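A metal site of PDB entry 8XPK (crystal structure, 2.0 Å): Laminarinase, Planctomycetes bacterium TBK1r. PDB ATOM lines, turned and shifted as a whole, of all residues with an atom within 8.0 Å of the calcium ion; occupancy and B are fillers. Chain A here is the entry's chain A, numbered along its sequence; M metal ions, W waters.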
ATOM      1  N   PRO A 117      -0.452  -4.376 -15.147  1.00  0.00           N
ATOM      2  CA  PRO A 117      -0.130  -5.560 -14.344  1.00  0.00           C
ATOM      3  C   PRO A 117      -1.251  -6.137 -13.464  1.00  0.00           C
ATOM      4  O   PRO A 117      -0.983  -6.900 -12.554  1.00  0.00           O
ATOM      5  CB  PRO A 117       0.949  -4.933 -13.482  1.00  0.00           C
ATOM      6  CG  PRO A 117       0.348  -3.629 -13.080  1.00  0.00           C
ATOM      7  CD  PRO A 117      -0.295  -3.132 -14.376  1.00  0.00           C
ATOM      8  N   LYS A 118      -2.487  -5.690 -13.713  1.00  0.00           N
ATOM      9  CA  LYS A 118      -3.623  -6.111 -12.930  1.00  0.00           C
ATOM     10  C   LYS A 118      -3.819  -7.618 -13.020  1.00  0.00           C
ATOM     11  O   LYS A 118      -4.354  -8.222 -12.092  1.00  0.00           O
ATOM     12  CB  LYS A 118      -4.892  -5.396 -13.409  1.00  0.00           C
ATOM     13  CG  LYS A 118      -5.084  -3.951 -12.957  1.00  0.00           C
ATOM     14  CD  LYS A 118      -5.924  -3.113 -13.921  1.00  0.00           C
ATOM     15  CE  LYS A 118      -6.393  -1.780 -13.408  1.00  0.00           C
ATOM     16  NZ  LYS A 118      -5.318  -0.952 -12.843  1.00  0.00           N
ATOM     17  N   CYS A 119      -3.321  -8.230 -14.119  1.00  0.00           N
ATOM     18  CA  CYS A 119      -3.431  -9.664 -14.320  1.00  0.00           C
ATOM     19  C   CYS A 119      -2.478 -10.412 -13.397  1.00  0.00           C
ATOM     20  O   CYS A 119      -2.621 -11.610 -13.181  1.00  0.00           O
ATOM     21  CB  CYS A 119      -3.137 -10.000 -15.768  1.00  0.00           C
ATOM     22  SG  CYS A 119      -1.481  -9.463 -16.271  1.00  0.00           S
ATOM     23  N   GLY A 120      -1.459  -9.734 -12.875  1.00  0.00           N
ATOM     24  CA  GLY A 120      -0.426 -10.392 -12.099  1.00  0.00           C
ATOM     25  C   GLY A 120       0.668 -10.947 -13.006  1.00  0.00           C
ATOM     26  O   GLY A 120       0.397 -11.367 -14.131  1.00  0.00           O
ATOM     27  N   PHE A 148       2.399  -6.456 -10.189  1.00  0.00           N
ATOM     28  CA  PHE A 148       0.972  -6.567  -9.927  1.00  0.00           C
ATOM     29  C   PHE A 148       0.417  -5.179  -9.676  1.00  0.00           C
ATOM     30  O   PHE A 148       1.166  -4.222  -9.612  1.00  0.00           O
ATOM     31  CB  PHE A 148       0.725  -7.518  -8.741  1.00  0.00           C
ATOM     32  CG  PHE A 148       1.397  -7.115  -7.434  1.00  0.00           C
ATOM     33  CD1 PHE A 148       2.730  -7.422  -7.184  1.00  0.00           C
ATOM     34  CD2 PHE A 148       0.685  -6.440  -6.445  1.00  0.00           C
ATOM     35  CE1 PHE A 148       3.341  -7.069  -5.986  1.00  0.00           C
ATOM     36  CE2 PHE A 148       1.287  -6.096  -5.237  1.00  0.00           C
ATOM     37  CZ  PHE A 148       2.624  -6.400  -5.018  1.00  0.00           C
ATOM     38  N   ALA A 149      -0.913  -5.105  -9.529  1.00  0.00           N
ATOM     39  CA  ALA A 149      -1.597  -3.897  -9.083  1.00  0.00           C
ATOM     40  C   ALA A 149      -1.670  -3.877  -7.555  1.00  0.00           C
ATOM     41  O   ALA A 149      -2.433  -4.625  -6.922  1.00  0.00           O
ATOM     42  CB  ALA A 149      -2.967  -3.801  -9.710  1.00  0.00           C
ATOM     43  N   GLY A 150      -0.860  -3.018  -6.951  1.00  0.00           N
ATOM     44  CA  GLY A 150      -0.658  -3.024  -5.516  1.00  0.00           C
ATOM     45  C   GLY A 150      -1.653  -2.135  -4.785  1.00  0.00           C
ATOM     46  O   GLY A 150      -2.827  -2.006  -5.159  1.00  0.00           O
ATOM     47  N   VAL A 151      -1.181  -1.526  -3.684  1.00  0.00           N
ATOM     48  CA  VAL A 151      -1.957  -0.518  -3.001  1.00  0.00           C
ATOM     49  C   VAL A 151      -2.333   0.513  -4.064  1.00  0.00           C
ATOM     50  O   VAL A 151      -1.546   0.798  -5.002  1.00  0.00           O
ATOM     51  CB  VAL A 151      -1.313   0.130  -1.754  1.00  0.00           C
ATOM     52  CG1 VAL A 151      -2.259   1.112  -1.081  1.00  0.00           C
ATOM     53  CG2 VAL A 151      -0.897  -0.884  -0.708  1.00  0.00           C
ATOM     54  N   GLY A 152      -3.591   0.970  -3.965  1.00  0.00           N
ATOM     55  CA  GLY A 152      -4.117   1.991  -4.864  1.00  0.00           C
ATOM     56  C   GLY A 152      -4.371   1.461  -6.268  1.00  0.00           C
ATOM     57  O   GLY A 152      -4.730   2.225  -7.169  1.00  0.00           O
ATOM     58  N   GLU A 153      -4.181   0.143  -6.430  1.00  0.00           N
ATOM     59  CA  GLU A 153      -4.290  -0.502  -7.728  1.00  0.00           C
ATOM     60  C   GLU A 153      -3.141  -0.066  -8.646  1.00  0.00           C
ATOM     61  O   GLU A 153      -3.242  -0.244  -9.862  1.00  0.00           O
ATOM     62  CB  GLU A 153      -5.642  -0.239  -8.405  1.00  0.00           C
ATOM     63  CG  GLU A 153      -6.816  -0.780  -7.591  1.00  0.00           C
ATOM     64  CD  GLU A 153      -6.726  -2.280  -7.337  1.00  0.00           C
ATOM     65  OE1 GLU A 153      -6.603  -3.013  -8.345  1.00  0.00           O
ATOM     66  OE2 GLU A 153      -6.723  -2.714  -6.164  1.00  0.00           O
ATOM     67  N   GLN A 154      -2.069   0.516  -8.068  1.00  0.00           N
ATOM     68  CA  GLN A 154      -1.023   1.068  -8.905  1.00  0.00           C
ATOM     69  C   GLN A 154       0.048   0.012  -9.130  1.00  0.00           C
ATOM     70  O   GLN A 154       0.334  -0.763  -8.226  1.00  0.00           O
ATOM     71  CB  GLN A 154      -0.422   2.318  -8.269  1.00  0.00           C
ATOM     72  CG  GLN A 154      -1.416   3.465  -8.201  1.00  0.00           C
ATOM     73  CD  GLN A 154      -2.187   3.623  -9.492  1.00  0.00           C
ATOM     74  OE1 GLN A 154      -3.400   3.320  -9.553  1.00  0.00           O
ATOM     75  NE2 GLN A 154      -1.509   4.020 -10.555  1.00  0.00           N
ATOM     76  N   THR A 156       3.011  -2.188  -9.053  1.00  0.00           N
ATOM     77  CA  THR A 156       3.952  -2.445  -7.969  1.00  0.00           C
ATOM     78  C   THR A 156       4.898  -3.543  -8.452  1.00  0.00           C
ATOM     79  O   THR A 156       4.403  -4.510  -9.026  1.00  0.00           O
ATOM     80  CB  THR A 156       3.219  -2.911  -6.708  1.00  0.00           C
ATOM     81  OG1 THR A 156       2.381  -1.853  -6.274  1.00  0.00           O
ATOM     82  CG2 THR A 156       4.151  -3.218  -5.546  1.00  0.00           C
ATOM     83  N   ALA A 200      -1.634 -10.833   1.287  1.00  0.00           N
ATOM     84  CA  ALA A 200      -2.128  -9.485   1.550  1.00  0.00           C
ATOM     85  C   ALA A 200      -3.225  -9.136   0.553  1.00  0.00           C
ATOM     86  O   ALA A 200      -3.214  -9.605  -0.576  1.00  0.00           O
ATOM     87  CB  ALA A 200      -0.980  -8.476   1.486  1.00  0.00           C
ATOM     88  N   SER A 201      -4.154  -8.280   0.997  1.00  0.00           N
ATOM     89  CA  SER A 201      -5.332  -7.918   0.226  1.00  0.00           C
ATOM     90  C   SER A 201      -4.986  -7.402  -1.173  1.00  0.00           C
ATOM     91  O   SER A 201      -5.772  -7.540  -2.114  1.00  0.00           O
ATOM     92  CB  SER A 201      -6.126  -6.889   0.998  1.00  0.00           C
ATOM     93  OG  SER A 201      -5.411  -5.664   1.152  1.00  0.00           O
ATOM     94  N   GLU A 202      -3.827  -6.748  -1.335  1.00  0.00           N
ATOM     95  CA  GLU A 202      -3.495  -6.144  -2.614  1.00  0.00           C
ATOM     96  C   GLU A 202      -2.964  -7.182  -3.590  1.00  0.00           C
ATOM     97  O   GLU A 202      -2.732  -6.851  -4.766  1.00  0.00           O
ATOM     98  CB  GLU A 202      -2.630  -4.896  -2.405  1.00  0.00           C
ATOM     99  CG  GLU A 202      -1.181  -5.138  -1.993  1.00  0.00           C
ATOM    100  CD  GLU A 202      -0.947  -5.188  -0.489  1.00  0.00           C
ATOM    101  OE1 GLU A 202      -1.914  -5.259   0.324  1.00  0.00           O
ATOM    102  OE2 GLU A 202       0.263  -5.125  -0.145  1.00  0.00           O
ATOM    103  N   MET A 203      -2.811  -8.447  -3.169  1.00  0.00           N
ATOM    104  CA  MET A 203      -2.161  -9.438  -4.008  1.00  0.00           C
ATOM    105  C   MET A 203      -3.106 -10.581  -4.390  1.00  0.00           C
ATOM    106  O   MET A 203      -2.668 -11.703  -4.688  1.00  0.00           O
ATOM    107  CB  MET A 203      -0.892  -9.995  -3.328  1.00  0.00           C
ATOM    108  CG  MET A 203       0.159  -8.926  -3.032  1.00  0.00           C
ATOM    109  SD  MET A 203       1.568  -9.574  -2.106  1.00  0.00           S
ATOM    110  CE  MET A 203       2.588 -10.176  -3.449  1.00  0.00           C
ATOM    111  N   LYS A 204      -4.409 -10.291  -4.453  1.00  0.00           N
ATOM    112  CA  LYS A 204      -5.370 -11.339  -4.775  1.00  0.00           C
ATOM    113  C   LYS A 204      -5.198 -11.840  -6.224  1.00  0.00           C
ATOM    114  O   LYS A 204      -5.626 -12.954  -6.524  1.00  0.00           O
ATOM    115  CB  LYS A 204      -6.838 -10.954  -4.520  1.00  0.00           C
ATOM    116  CG  LYS A 204      -7.110 -10.666  -3.043  1.00  0.00           C
ATOM    117  CD  LYS A 204      -8.449 -10.020  -2.670  1.00  0.00           C
ATOM    118  CE  LYS A 204      -8.450  -9.519  -1.238  1.00  0.00           C
ATOM    119  NZ  LYS A 204      -9.750  -9.608  -0.564  1.00  0.00           N
ATOM    120  N   GLU A 205      -4.567 -11.054  -7.092  1.00  0.00           N
ATOM    121  CA  GLU A 205      -4.297 -11.477  -8.466  1.00  0.00           C
ATOM    122  C   GLU A 205      -3.437 -12.750  -8.514  1.00  0.00           C
ATOM    123  O   GLU A 205      -3.330 -13.364  -9.563  1.00  0.00           O
ATOM    124  CB  GLU A 205      -3.401 -10.578  -9.310  1.00  0.00           C
ATOM    125  CG  GLU A 205      -3.785  -9.122  -9.385  1.00  0.00           C
ATOM    126  CD  GLU A 205      -3.306  -8.254  -8.244  1.00  0.00           C
ATOM    127  OE1 GLU A 205      -3.619  -8.601  -7.095  1.00  0.00           O
ATOM    128  OE2 GLU A 205      -2.773  -7.159  -8.558  1.00  0.00           O
ATOM    129  N   TYR A 206      -2.797 -13.124  -7.384  1.00  0.00           N
ATOM    130  CA  TYR A 206      -1.940 -14.304  -7.356  1.00  0.00           C
ATOM    131  C   TYR A 206      -2.719 -15.544  -6.920  1.00  0.00           C
ATOM    132  O   TYR A 206      -2.106 -16.560  -6.639  1.00  0.00           O
ATOM    133  CB  TYR A 206      -0.707 -14.098  -6.478  1.00  0.00           C
ATOM    134  CG  TYR A 206       0.261 -13.131  -7.130  1.00  0.00           C
ATOM    135  CD1 TYR A 206       0.928 -13.473  -8.296  1.00  0.00           C
ATOM    136  CD2 TYR A 206       0.432 -11.844  -6.635  1.00  0.00           C
ATOM    137  CE1 TYR A 206       1.779 -12.585  -8.926  1.00  0.00           C
ATOM    138  CE2 TYR A 206       1.287 -10.948  -7.254  1.00  0.00           C
ATOM    139  CZ  TYR A 206       1.963 -11.323  -8.406  1.00  0.00           C
ATOM    140  OH  TYR A 206       2.792 -10.452  -9.034  1.00  0.00           O
HETATM  141 CA    CA M   1      -3.918  -6.247  -6.552  1.00  0.00          CA
HETATM  142  O   HOH W   1      -5.485  -5.680  -7.953  1.00  0.00           O
HETATM  143  O   HOH W   2      -4.741  -4.248  -5.374  1.00  0.00           O
HETATM  144  O   HOH W   3      -5.632  -7.280  -4.884  1.00  0.00           O
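The calcium ion is bound by water W1 (2.2 Å), the backbone carbonyl oxygen (O) of Glu 202 (2.2 Å), the backbone carbonyl oxygen (O) of Ala 149 (2.2 Å), the side-chain carboxylate (OE1) of Glu 205 (2.4 Å), water W2 (2.5 Å), the side-chain carboxylate (OE2) of Glu 205 (2.5 Å) and water W3 (2.6 Å).
The calcium ion has seven donor atoms within binding distance.
Water W2 lies within hydrogen-bond range of OE2 of Glu 153 (2.6 Å) and O of Gly 150 (3.0 Å).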
